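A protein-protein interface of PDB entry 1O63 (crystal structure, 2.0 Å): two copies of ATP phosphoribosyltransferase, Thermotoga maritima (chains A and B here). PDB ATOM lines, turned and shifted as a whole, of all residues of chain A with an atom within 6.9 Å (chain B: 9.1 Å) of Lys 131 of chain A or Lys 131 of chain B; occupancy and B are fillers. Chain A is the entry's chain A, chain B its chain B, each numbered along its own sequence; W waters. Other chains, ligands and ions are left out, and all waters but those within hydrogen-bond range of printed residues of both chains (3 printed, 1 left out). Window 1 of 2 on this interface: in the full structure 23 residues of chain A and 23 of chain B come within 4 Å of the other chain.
Among the printed residues, 14 pairs touch across the chains. Among the printed residues, no Asp or Glu carboxylate lies within 4 Å of a Lys or Arg side-chain nitrogen of the other chain.
O of Thr 108 of chain B lies within hydrogen-bond range of N of Leu 130 of chain B (2.8 Å). O of Thr 108 of chain A is in hydrogen-bond range of N of Leu 130 of chain A, at 2.8 Å.
Arg 46 of chain A touches Gly 132 of chain B, and with the chains exchanged Gly 132 of chain A touches Arg 46 of chain B. Phe 48 of chain A touches Lys 131 of chain B, and with the chains exchanged Lys 131 of chain A touches Phe 48 of chain B. Asp 49 of chain A touches Leu 130 of chain B, and with the chains exchanged Leu 130 of chain A touches Asp 49 of chain B. Asp 49 of chain A touches Lys 131 of chain B, and with the chains exchanged Lys 131 of chain A touches Asp 49 of chain B.
Printed residues of chain A within 4 Å of Lys 131 of chain B: Arg 46, Phe 48, Asp 49 and Lys 131. Gly 132 of chain A touches just these residues of chain B: Arg 46 (3.6 Å) and Asp 49 (3.6 Å). Printed residues of chain A within 4 Å of Leu 130 of chain B: Asp 49. Of the printed residues of chain B, Asp 49 of chain A touches Leu 130, Lys 131 and Gly 132. Ser 133 of chain A touches none of the printed residues of chain B. Pro 129 of chain B touches none of the printed residues of chain A. The nearest residue of chain B that does not touch Lys 131 of chain A is Pro 47 of chain B (6.4 Å). The nearest residue of chain A that does not touch Lys 131 of chain B is Pro 47 of chain A (6.4 Å). The nearest printed residue of chain A that does not touch Thr 52 of chain B is Pro 129 of chain A (4.2 Å).
Water W1 lies within hydrogen-bond range of the side-chain carboxylate of Asp 49 of chain A (2.4 Å), the backbone carbonyl oxygen of Gly 132 of chain B (2.7 Å) and the backbone NH of Arg 46 of chain A (3.2 Å). Water W3 lies within hydrogen-bond range of the side-chain hydroxyl (OH) of Tyr 53 of chain B (2.6 Å) and the backbone carbonyl oxygen (O) of Ser 133 of chain A (2.8 Å). Water W2 lies within hydrogen-bond range of OD2 of Asp 49 of chain A (2.7 Å) and O of Pro 129 of chain B (2.8 Å).
The backbone NH of Lys 131 of chain A lies within hydrogen-bond range of the side-chain carboxylate of Asp 49 of chain B (2.9 Å). The side-chain carboxylate (OD1) of Asp 49 of chain A sits at hydrogen-bond distance from the backbone NH (N) of Lys 131 of chain B, 2.9 Å away.
Among the printed residues, merely in contact across the chains: Asp 49 of chain A with Leu 130 of chain B (3.3 Å), Leu 130 of chain A with Asp 49 of chain B (3.4 Å), Arg 46 of chain A with Gly 132 of chain B (3.6 Å), Gly 132 of chain A with Asp 49 of chain B (3.6 Å), Gly 132 of chain A with Arg 46 of chain B (3.6 Å), Asp 49 of chain A with Gly 132 of chain B (3.6 Å), Leu 130 of chain A with Thr 52 of chain B (3.7 Å), Lys 131 of chain A with Phe 48 of chain B (3.8 Å), Arg 46 of chain A with Lys 131 of chain B (3.8 Å), Lys 131 of chain A with Arg 46 of chain B (3.9 Å), Lys 131 of chain A with Lys 131 of chain B (3.9 Å) and Phe 48 of chain A with Lys 131 of chain B (3.95 Å).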
ATOM      1  N   ARG A  46      -1.833 -13.874  39.754  1.00  0.00           N
ATOM      2  CA  ARG A  46      -2.295 -13.003  38.660  1.00  0.00           C
ATOM      3  C   ARG A  46      -3.737 -12.599  38.978  1.00  0.00           C
ATOM      4  O   ARG A  46      -4.513 -13.398  39.519  1.00  0.00           O
ATOM      5  CB  ARG A  46      -2.215 -13.680  37.329  1.00  0.00           C
ATOM      6  CG  ARG A  46      -0.903 -14.225  36.841  1.00  0.00           C
ATOM      7  CD  ARG A  46       0.219 -13.222  36.830  1.00  0.00           C
ATOM      8  NE  ARG A  46      -0.151 -11.898  36.352  1.00  0.00           N
ATOM      9  CZ  ARG A  46       0.656 -10.840  36.481  1.00  0.00           C
ATOM     10  NH1 ARG A  46       0.286  -9.650  36.029  1.00  0.00           N
ATOM     11  NH2 ARG A  46       1.849 -10.994  37.053  1.00  0.00           N
ATOM     12  N   PRO A  47      -4.084 -11.355  38.675  1.00  0.00           N
ATOM     13  CA  PRO A  47      -5.389 -10.797  38.978  1.00  0.00           C
ATOM     14  C   PRO A  47      -6.556 -11.653  38.614  1.00  0.00           C
ATOM     15  O   PRO A  47      -7.493 -11.865  39.437  1.00  0.00           O
ATOM     16  CB  PRO A  47      -5.398  -9.487  38.143  1.00  0.00           C
ATOM     17  CG  PRO A  47      -3.953  -9.071  38.152  1.00  0.00           C
ATOM     18  CD  PRO A  47      -3.187 -10.367  38.030  1.00  0.00           C
ATOM     19  N   PHE A  48      -6.558 -12.261  37.423  1.00  0.00           N
ATOM     20  CA  PHE A  48      -7.660 -13.123  37.013  1.00  0.00           C
ATOM     21  C   PHE A  48      -7.710 -14.422  37.790  1.00  0.00           C
ATOM     22  O   PHE A  48      -8.776 -15.059  37.850  1.00  0.00           O
ATOM     23  CB  PHE A  48      -7.594 -13.423  35.494  1.00  0.00           C
ATOM     24  CG  PHE A  48      -8.496 -12.459  34.743  1.00  0.00           C
ATOM     25  CD1 PHE A  48      -8.016 -11.221  34.350  1.00  0.00           C
ATOM     26  CD2 PHE A  48      -9.813 -12.774  34.485  1.00  0.00           C
ATOM     27  CE1 PHE A  48      -8.829 -10.322  33.682  1.00  0.00           C
ATOM     28  CE2 PHE A  48     -10.627 -11.880  33.824  1.00  0.00           C
ATOM     29  CZ  PHE A  48     -10.137 -10.643  33.409  1.00  0.00           C
ATOM     30  N   ASP A  49      -6.655 -14.775  38.499  1.00  0.00           N
ATOM     31  CA  ASP A  49      -6.652 -16.006  39.296  1.00  0.00           C
ATOM     32  C   ASP A  49      -7.151 -15.777  40.712  1.00  0.00           C
ATOM     33  O   ASP A  49      -7.317 -16.739  41.450  1.00  0.00           O
ATOM     34  CB  ASP A  49      -5.234 -16.590  39.342  1.00  0.00           C
ATOM     35  CG  ASP A  49      -4.769 -17.072  37.976  1.00  0.00           C
ATOM     36  OD1 ASP A  49      -3.553 -17.113  37.736  1.00  0.00           O
ATOM     37  OD2 ASP A  49      -5.613 -17.394  37.126  1.00  0.00           O
ATOM     38  N   THR A 108     -10.198  -7.536  21.830  1.00  0.00           N
ATOM     39  CA  THR A 108     -10.226  -7.213  23.272  1.00  0.00           C
ATOM     40  C   THR A 108      -9.606  -8.360  24.065  1.00  0.00           C
ATOM     41  O   THR A 108      -9.575  -9.494  23.568  1.00  0.00           O
ATOM     42  CB  THR A 108     -11.704  -7.047  23.709  1.00  0.00           C
ATOM     43  OG1 THR A 108     -11.793  -6.756  25.100  1.00  0.00           O
ATOM     44  CG2 THR A 108     -12.482  -8.341  23.444  1.00  0.00           C
ATOM     45  N   LYS A 109      -9.173  -8.083  25.276  1.00  0.00           N
ATOM     46  CA  LYS A 109      -8.777  -9.089  26.245  1.00  0.00           C
ATOM     47  C   LYS A 109      -9.984  -9.501  27.101  1.00  0.00           C
ATOM     48  O   LYS A 109      -9.891 -10.408  27.949  1.00  0.00           O
ATOM     49  CB  LYS A 109      -7.724  -8.556  27.229  1.00  0.00           C
ATOM     50  CG  LYS A 109      -6.481  -8.004  26.564  1.00  0.00           C
ATOM     51  CD  LYS A 109      -5.329  -7.915  27.548  1.00  0.00           C
ATOM     52  CE  LYS A 109      -5.376  -6.642  28.332  1.00  0.00           C
ATOM     53  NZ  LYS A 109      -4.094  -6.354  29.047  1.00  0.00           N
ATOM     54  N   PRO A 129     -10.483 -12.124  20.599  1.00  0.00           N
ATOM     55  CA  PRO A 129      -9.733 -12.152  21.824  1.00  0.00           C
ATOM     56  C   PRO A 129      -8.231 -12.009  21.621  1.00  0.00           C
ATOM     57  O   PRO A 129      -7.664 -12.701  20.777  1.00  0.00           O
ATOM     58  CB  PRO A 129     -10.001 -13.531  22.431  1.00  0.00           C
ATOM     59  CG  PRO A 129     -11.141 -14.085  21.684  1.00  0.00           C
ATOM     60  CD  PRO A 129     -11.112 -13.446  20.315  1.00  0.00           C
ATOM     61  N   LEU A 130      -7.617 -11.126  22.382  1.00  0.00           N
ATOM     62  CA  LEU A 130      -6.163 -10.897  22.307  1.00  0.00           C
ATOM     63  C   LEU A 130      -5.617 -10.963  23.735  1.00  0.00           C
ATOM     64  O   LEU A 130      -6.379 -10.692  24.688  1.00  0.00           O
ATOM     65  CB  LEU A 130      -5.878  -9.510  21.725  1.00  0.00           C
ATOM     66  CG  LEU A 130      -6.164  -9.310  20.238  1.00  0.00           C
ATOM     67  CD1 LEU A 130      -5.815  -7.892  19.791  1.00  0.00           C
ATOM     68  CD2 LEU A 130      -5.378 -10.328  19.410  1.00  0.00           C
ATOM     69  N   LYS A 131      -4.309 -11.128  23.869  1.00  0.00           N
ATOM     70  CA  LYS A 131      -3.708 -11.207  25.196  1.00  0.00           C
ATOM     71  C   LYS A 131      -3.093  -9.892  25.631  1.00  0.00           C
ATOM     72  O   LYS A 131      -2.713  -9.758  26.788  1.00  0.00           O
ATOM     73  CB  LYS A 131      -2.630 -12.292  25.243  1.00  0.00           C
ATOM     74  CG  LYS A 131      -3.043 -13.653  24.735  1.00  0.00           C
ATOM     75  CD  LYS A 131      -3.470 -14.556  25.898  1.00  0.00           C
ATOM     76  CE  LYS A 131      -4.926 -14.299  26.245  1.00  0.00           C
ATOM     77  NZ  LYS A 131      -5.235 -14.663  27.664  1.00  0.00           N
ATOM     78  N   GLY A 132      -2.848  -8.973  24.714  1.00  0.00           N
ATOM     79  CA  GLY A 132      -2.233  -7.686  25.100  1.00  0.00           C
ATOM     80  C   GLY A 132      -1.976  -6.896  23.811  1.00  0.00           C
ATOM     81  O   GLY A 132      -2.402  -7.360  22.747  1.00  0.00           O
ATOM     82  N   SER A 133      -1.431  -5.703  23.943  1.00  0.00           N
ATOM     83  CA  SER A 133      -1.177  -4.821  22.813  1.00  0.00           C
ATOM     84  C   SER A 133      -2.397  -4.736  21.901  1.00  0.00           C
ATOM     85  O   SER A 133      -2.309  -4.663  20.669  1.00  0.00           O
ATOM     86  CB  SER A 133       0.057  -5.287  22.033  1.00  0.00           C
ATOM     87  OG  SER A 133       1.223  -5.188  22.831  1.00  0.00           O
ATOM     88  N   VAL A 134      -3.576  -4.578  22.529  1.00  0.00           N
ATOM     89  CA  VAL A 134      -4.826  -4.566  21.794  1.00  0.00           C
ATOM     90  C   VAL A 134      -4.910  -3.354  20.887  1.00  0.00           C
ATOM     91  O   VAL A 134      -5.618  -3.372  19.882  1.00  0.00           O
ATOM     92  CB  VAL A 134      -6.036  -4.651  22.735  1.00  0.00           C
ATOM     93  CG1 VAL A 134      -7.332  -4.733  21.948  1.00  0.00           C
ATOM     94  CG2 VAL A 134      -5.928  -5.920  23.615  1.00  0.00           C
ATOM     95  N   VAL B  45       3.404  -8.757  18.379  1.00  0.00           N
ATOM     96  CA  VAL B  45       2.253  -9.119  19.204  1.00  0.00           C
ATOM     97  C   VAL B  45       2.631 -10.116  20.280  1.00  0.00           C
ATOM     98  O   VAL B  45       3.725 -10.679  20.232  1.00  0.00           O
ATOM     99  CB  VAL B  45       1.168  -9.744  18.292  1.00  0.00           C
ATOM    100  CG1 VAL B  45       0.709  -8.736  17.233  1.00  0.00           C
ATOM    101  CG2 VAL B  45       1.698 -10.997  17.614  1.00  0.00           C
ATOM    102  N   ARG B  46       1.693 -10.383  21.200  1.00  0.00           N
ATOM    103  CA  ARG B  46       1.924 -11.440  22.190  1.00  0.00           C
ATOM    104  C   ARG B  46       2.012 -12.789  21.468  1.00  0.00           C
ATOM    105  O   ARG B  46       1.230 -13.067  20.559  1.00  0.00           O
ATOM    106  CB  ARG B  46       0.805 -11.477  23.224  1.00  0.00           C
ATOM    107  CG  ARG B  46       0.489 -10.138  23.883  1.00  0.00           C
ATOM    108  CD  ARG B  46       1.726  -9.411  24.334  1.00  0.00           C
ATOM    109  NE  ARG B  46       2.591 -10.207  25.186  1.00  0.00           N
ATOM    110  CZ  ARG B  46       2.271 -10.729  26.361  1.00  0.00           C
ATOM    111  NH1 ARG B  46       3.179 -11.424  27.053  1.00  0.00           N
ATOM    112  NH2 ARG B  46       1.054 -10.570  26.864  1.00  0.00           N
ATOM    113  N   PRO B  47       2.917 -13.658  21.893  1.00  0.00           N
ATOM    114  CA  PRO B  47       3.066 -14.975  21.287  1.00  0.00           C
ATOM    115  C   PRO B  47       1.773 -15.692  21.087  1.00  0.00           C
ATOM    116  O   PRO B  47       1.520 -16.208  19.978  1.00  0.00           O
ATOM    117  CB  PRO B  47       4.014 -15.710  22.238  1.00  0.00           C
ATOM    118  CG  PRO B  47       4.846 -14.617  22.814  1.00  0.00           C
ATOM    119  CD  PRO B  47       3.901 -13.440  22.976  1.00  0.00           C
ATOM    120  N   PHE B  48       0.855 -15.693  22.071  1.00  0.00           N
ATOM    121  CA  PHE B  48      -0.419 -16.369  21.880  1.00  0.00           C
ATOM    122  C   PHE B  48      -1.314 -15.705  20.853  1.00  0.00           C
ATOM    123  O   PHE B  48      -2.240 -16.355  20.365  1.00  0.00           O
ATOM    124  CB  PHE B  48      -1.184 -16.560  23.210  1.00  0.00           C
ATOM    125  CG  PHE B  48      -0.910 -17.926  23.801  1.00  0.00           C
ATOM    126  CD1 PHE B  48       0.299 -18.183  24.422  1.00  0.00           C
ATOM    127  CD2 PHE B  48      -1.824 -18.949  23.686  1.00  0.00           C
ATOM    128  CE1 PHE B  48       0.587 -19.429  24.952  1.00  0.00           C
ATOM    129  CE2 PHE B  48      -1.551 -20.201  24.216  1.00  0.00           C
ATOM    130  CZ  PHE B  48      -0.356 -20.441  24.858  1.00  0.00           C
ATOM    131  N   ASP B  49      -1.081 -14.449  20.507  1.00  0.00           N
ATOM    132  CA  ASP B  49      -1.885 -13.793  19.470  1.00  0.00           C
ATOM    133  C   ASP B  49      -1.354 -14.035  18.067  1.00  0.00           C
ATOM    134  O   ASP B  49      -2.014 -13.644  17.097  1.00  0.00           O
ATOM    135  CB  ASP B  49      -1.930 -12.274  19.754  1.00  0.00           C
ATOM    136  CG  ASP B  49      -2.625 -11.993  21.088  1.00  0.00           C
ATOM    137  OD1 ASP B  49      -3.466 -12.820  21.468  1.00  0.00           O
ATOM    138  OD2 ASP B  49      -2.297 -10.977  21.745  1.00  0.00           O
ATOM    139  N   VAL B  50      -0.177 -14.642  17.902  1.00  0.00           N
ATOM    140  CA  VAL B  50       0.377 -14.854  16.556  1.00  0.00           C
ATOM    141  C   VAL B  50      -0.592 -15.567  15.638  1.00  0.00           C
ATOM    142  O   VAL B  50      -0.983 -15.031  14.591  1.00  0.00           O
ATOM    143  CB  VAL B  50       1.743 -15.552  16.579  1.00  0.00           C
ATOM    144  CG1 VAL B  50       2.170 -16.001  15.176  1.00  0.00           C
ATOM    145  CG2 VAL B  50       2.800 -14.629  17.167  1.00  0.00           C
ATOM    146  N   PRO B  51      -1.088 -16.740  16.007  1.00  0.00           N
ATOM    147  CA  PRO B  51      -2.067 -17.461  15.209  1.00  0.00           C
ATOM    148  C   PRO B  51      -3.332 -16.680  14.936  1.00  0.00           C
ATOM    149  O   PRO B  51      -3.852 -16.736  13.815  1.00  0.00           O
ATOM    150  CB  PRO B  51      -2.366 -18.717  16.015  1.00  0.00           C
ATOM    151  CG  PRO B  51      -1.180 -18.905  16.887  1.00  0.00           C
ATOM    152  CD  PRO B  51      -0.689 -17.507  17.201  1.00  0.00           C
ATOM    153  N   THR B  52      -3.818 -15.863  15.882  1.00  0.00           N
ATOM    154  CA  THR B  52      -5.026 -15.088  15.637  1.00  0.00           C
ATOM    155  C   THR B  52      -4.813 -14.012  14.594  1.00  0.00           C
ATOM    156  O   THR B  52      -5.728 -13.733  13.798  1.00  0.00           O
ATOM    157  CB  THR B  52      -5.775 -14.593  16.863  1.00  0.00           C
ATOM    158  OG1 THR B  52      -5.710 -13.192  17.086  1.00  0.00           O
ATOM    159  CG2 THR B  52      -5.424 -15.353  18.118  1.00  0.00           C
ATOM    160  N   TYR B  53      -3.586 -13.493  14.470  1.00  0.00           N
ATOM    161  CA  TYR B  53      -3.311 -12.535  13.387  1.00  0.00           C
ATOM    162  C   TYR B  53      -3.232 -13.267  12.040  1.00  0.00           C
ATOM    163  O   TYR B  53      -3.567 -12.690  10.997  1.00  0.00           O
ATOM    164  CB  TYR B  53      -2.028 -11.765  13.662  1.00  0.00           C
ATOM    165  CG  TYR B  53      -2.242 -10.487  14.457  1.00  0.00           C
ATOM    166  CD1 TYR B  53      -2.557 -10.525  15.802  1.00  0.00           C
ATOM    167  CD2 TYR B  53      -2.097  -9.240  13.854  1.00  0.00           C
ATOM    168  CE1 TYR B  53      -2.752  -9.355  16.538  1.00  0.00           C
ATOM    169  CE2 TYR B  53      -2.314  -8.081  14.560  1.00  0.00           C
ATOM    170  CZ  TYR B  53      -2.637  -8.141  15.907  1.00  0.00           C
ATOM    171  OH  TYR B  53      -2.803  -6.977  16.595  1.00  0.00           O
ATOM    172  N   VAL B  68       2.133 -22.606  21.980  1.00  0.00           N
ATOM    173  CA  VAL B  68       0.983 -21.875  21.417  1.00  0.00           C
ATOM    174  C   VAL B  68       0.205 -22.749  20.455  1.00  0.00           C
ATOM    175  O   VAL B  68      -1.038 -22.789  20.510  1.00  0.00           O
ATOM    176  CB  VAL B  68       1.457 -20.607  20.675  1.00  0.00           C
ATOM    177  CG1 VAL B  68       0.357 -19.994  19.810  1.00  0.00           C
ATOM    178  CG2 VAL B  68       1.956 -19.567  21.670  1.00  0.00           C
ATOM    179  N   ALA B 107      -3.180 -27.836  37.827  1.00  0.00           N
ATOM    180  CA  ALA B 107      -3.288 -26.413  37.514  1.00  0.00           C
ATOM    181  C   ALA B 107      -2.384 -26.121  36.310  1.00  0.00           C
ATOM    182  O   ALA B 107      -1.313 -26.698  36.192  1.00  0.00           O
ATOM    183  CB  ALA B 107      -2.816 -25.599  38.705  1.00  0.00           C
ATOM    184  N   THR B 108      -2.860 -25.247  35.402  1.00  0.00           N
ATOM    185  CA  THR B 108      -2.010 -25.044  34.213  1.00  0.00           C
ATOM    186  C   THR B 108      -2.443 -23.772  33.494  1.00  0.00           C
ATOM    187  O   THR B 108      -3.577 -23.330  33.660  1.00  0.00           O
ATOM    188  CB  THR B 108      -2.240 -26.241  33.256  1.00  0.00           C
ATOM    189  OG1 THR B 108      -1.434 -26.116  32.090  1.00  0.00           O
ATOM    190  CG2 THR B 108      -3.709 -26.301  32.827  1.00  0.00           C
ATOM    191  N   LYS B 109      -1.557 -23.253  32.670  1.00  0.00           N
ATOM    192  CA  LYS B 109      -1.894 -22.127  31.792  1.00  0.00           C
ATOM    193  C   LYS B 109      -2.267 -22.720  30.426  1.00  0.00           C
ATOM    194  O   LYS B 109      -2.683 -22.015  29.534  1.00  0.00           O
ATOM    195  CB  LYS B 109      -0.645 -21.243  31.562  1.00  0.00           C
ATOM    196  CG  LYS B 109      -0.486 -20.190  32.659  1.00  0.00           C
ATOM    197  CD  LYS B 109       0.969 -19.736  32.740  1.00  0.00           C
ATOM    198  CE  LYS B 109       1.382 -19.018  31.458  1.00  0.00           C
ATOM    199  NZ  LYS B 109       2.872 -18.723  31.570  1.00  0.00           N
ATOM    200  N   PHE B 110      -2.119 -24.058  30.325  1.00  0.00           N
ATOM    201  CA  PHE B 110      -2.359 -24.776  29.081  1.00  0.00           C
ATOM    202  C   PHE B 110      -3.371 -25.920  29.276  1.00  0.00           C
ATOM    203  O   PHE B 110      -2.993 -27.103  29.356  1.00  0.00           O
ATOM    204  CB  PHE B 110      -1.035 -25.385  28.562  1.00  0.00           C
ATOM    205  CG  PHE B 110       0.091 -24.368  28.542  1.00  0.00           C
ATOM    206  CD1 PHE B 110       0.210 -23.448  27.518  1.00  0.00           C
ATOM    207  CD2 PHE B 110       0.966 -24.290  29.605  1.00  0.00           C
ATOM    208  CE1 PHE B 110       1.232 -22.507  27.515  1.00  0.00           C
ATOM    209  CE2 PHE B 110       1.999 -23.361  29.613  1.00  0.00           C
ATOM    210  CZ  PHE B 110       2.123 -22.459  28.579  1.00  0.00           C
ATOM    211  N   PRO B 111      -4.635 -25.570  29.403  1.00  0.00           N
ATOM    212  CA  PRO B 111      -5.699 -26.506  29.696  1.00  0.00           C
ATOM    213  C   PRO B 111      -5.998 -27.471  28.588  1.00  0.00           C
ATOM    214  O   PRO B 111      -6.288 -28.662  28.868  1.00  0.00           O
ATOM    215  CB  PRO B 111      -6.870 -25.632  30.100  1.00  0.00           C
ATOM    216  CG  PRO B 111      -6.613 -24.301  29.473  1.00  0.00           C
ATOM    217  CD  PRO B 111      -5.124 -24.156  29.419  1.00  0.00           C
ATOM    218  N   ILE B 128      -7.438 -26.931  36.440  1.00  0.00           N
ATOM    219  CA  ILE B 128      -7.662 -25.578  36.983  1.00  0.00           C
ATOM    220  C   ILE B 128      -6.798 -24.591  36.214  1.00  0.00           C
ATOM    221  O   ILE B 128      -5.592 -24.487  36.434  1.00  0.00           O
ATOM    222  CB  ILE B 128      -7.282 -25.556  38.481  1.00  0.00           C
ATOM    223  CG1 ILE B 128      -8.193 -26.541  39.236  1.00  0.00           C
ATOM    224  CG2 ILE B 128      -7.421 -24.157  39.091  1.00  0.00           C
ATOM    225  CD1 ILE B 128      -7.581 -27.064  40.523  1.00  0.00           C
ATOM    226  N   PRO B 129      -7.374 -23.881  35.259  1.00  0.00           N
ATOM    227  CA  PRO B 129      -6.615 -22.945  34.442  1.00  0.00           C
ATOM    228  C   PRO B 129      -6.132 -21.763  35.250  1.00  0.00           C
ATOM    229  O   PRO B 129      -6.903 -21.281  36.100  1.00  0.00           O
ATOM    230  CB  PRO B 129      -7.610 -22.464  33.384  1.00  0.00           C
ATOM    231  CG  PRO B 129      -8.848 -23.203  33.572  1.00  0.00           C
ATOM    232  CD  PRO B 129      -8.809 -23.876  34.918  1.00  0.00           C
ATOM    233  N   LEU B 130      -4.875 -21.358  35.071  1.00  0.00           N
ATOM    234  CA  LEU B 130      -4.397 -20.146  35.744  1.00  0.00           C
ATOM    235  C   LEU B 130      -3.730 -19.282  34.660  1.00  0.00           C
ATOM    236  O   LEU B 130      -3.523 -19.799  33.552  1.00  0.00           O
ATOM    237  CB  LEU B 130      -3.397 -20.429  36.872  1.00  0.00           C
ATOM    238  CG  LEU B 130      -3.947 -21.261  38.055  1.00  0.00           C
ATOM    239  CD1 LEU B 130      -2.803 -21.802  38.915  1.00  0.00           C
ATOM    240  CD2 LEU B 130      -4.886 -20.421  38.917  1.00  0.00           C
ATOM    241  N   LYS B 131      -3.343 -18.071  35.008  1.00  0.00           N
ATOM    242  CA  LYS B 131      -2.714 -17.181  34.036  1.00  0.00           C
ATOM    243  C   LYS B 131      -1.215 -17.083  34.284  1.00  0.00           C
ATOM    244  O   LYS B 131      -0.487 -16.580  33.442  1.00  0.00           O
ATOM    245  CB  LYS B 131      -3.306 -15.770  34.091  1.00  0.00           C
ATOM    246  CG  LYS B 131      -4.814 -15.731  33.893  1.00  0.00           C
ATOM    247  CD  LYS B 131      -5.140 -16.016  32.436  1.00  0.00           C
ATOM    248  CE  LYS B 131      -6.623 -15.808  32.150  1.00  0.00           C
ATOM    249  NZ  LYS B 131      -6.937 -16.371  30.790  1.00  0.00           N
ATOM    250  N   GLY B 132      -0.749 -17.498  35.461  1.00  0.00           N
ATOM    251  CA  GLY B 132       0.712 -17.361  35.704  1.00  0.00           C
ATOM    252  C   GLY B 132       1.036 -17.872  37.107  1.00  0.00           C
ATOM    253  O   GLY B 132       0.138 -18.343  37.810  1.00  0.00           O
ATOM    254  N   SER B 133       2.319 -17.958  37.417  1.00  0.00           N
ATOM    255  CA  SER B 133       2.794 -18.422  38.712  1.00  0.00           C
ATOM    256  C   SER B 133       2.117 -19.741  39.104  1.00  0.00           C
ATOM    257  O   SER B 133       1.670 -19.916  40.240  1.00  0.00           O
ATOM    258  CB  SER B 133       2.542 -17.386  39.796  1.00  0.00           C
ATOM    259  OG  SER B 133       3.395 -16.265  39.685  1.00  0.00           O
ATOM    260  N   VAL B 134       2.123 -20.674  38.166  1.00  0.00           N
ATOM    261  CA  VAL B 134       1.470 -21.952  38.289  1.00  0.00           C
ATOM    262  C   VAL B 134       2.108 -22.802  39.392  1.00  0.00           C
ATOM    263  O   VAL B 134       1.415 -23.567  40.043  1.00  0.00           O
ATOM    264  CB  VAL B 134       1.428 -22.727  36.966  1.00  0.00           C
ATOM    265  CG1 VAL B 134       0.692 -24.060  37.145  1.00  0.00           C
ATOM    266  CG2 VAL B 134       0.677 -21.913  35.886  1.00  0.00           C
ATOM    267  N   GLU B 135       3.394 -22.612  39.670  1.00  0.00           N
ATOM    268  CA  GLU B 135       4.064 -23.365  40.730  1.00  0.00           C
ATOM    269  C   GLU B 135       3.455 -23.096  42.103  1.00  0.00           C
ATOM    270  O   GLU B 135       3.556 -23.959  42.994  1.00  0.00           O
ATOM    271  CB  GLU B 135       5.560 -23.110  40.747  1.00  0.00           C
ATOM    272  CG  GLU B 135       5.993 -21.739  41.265  1.00  0.00           C
ATOM    273  CD  GLU B 135       5.867 -20.653  40.205  1.00  0.00           C
ATOM    274  OE1 GLU B 135       5.458 -20.924  39.068  1.00  0.00           O
ATOM    275  OE2 GLU B 135       6.229 -19.504  40.518  1.00  0.00           O
ATOM    276  N   LEU B 142      -4.103 -25.835  45.940  1.00  0.00           N
ATOM    277  CA  LEU B 142      -5.051 -25.681  44.853  1.00  0.00           C
ATOM    278  C   LEU B 142      -5.022 -26.901  43.947  1.00  0.00           C
ATOM    279  O   LEU B 142      -6.053 -27.302  43.384  1.00  0.00           O
ATOM    280  CB  LEU B 142      -4.766 -24.398  44.054  1.00  0.00           C
ATOM    281  CG  LEU B 142      -5.688 -24.072  42.889  1.00  0.00           C
ATOM    282  CD1 LEU B 142      -7.158 -23.983  43.288  1.00  0.00           C
ATOM    283  CD2 LEU B 142      -5.260 -22.771  42.194  1.00  0.00           C
ATOM    284  N   ASP B 148       3.373 -27.221  33.122  1.00  0.00           N
ATOM    285  CA  ASP B 148       3.855 -25.873  32.831  1.00  0.00           C
ATOM    286  C   ASP B 148       5.206 -25.951  32.122  1.00  0.00           C
ATOM    287  O   ASP B 148       5.730 -27.041  31.889  1.00  0.00           O
ATOM    288  CB  ASP B 148       4.037 -25.112  34.153  1.00  0.00           C
ATOM    289  CG  ASP B 148       4.111 -23.609  33.997  1.00  0.00           C
ATOM    290  OD1 ASP B 148       3.877 -23.051  32.890  1.00  0.00           O
ATOM    291  OD2 ASP B 148       4.469 -22.964  35.015  1.00  0.00           O
HETATM  292  O   HOH W   1      -1.723 -17.017  39.331  1.00  0.00           O
HETATM  293  O   HOH W   2      -7.910 -18.820  36.829  1.00  0.00           O
HETATM  294  O   HOH W   3      -2.118  -6.988  19.064  1.00  0.00           O
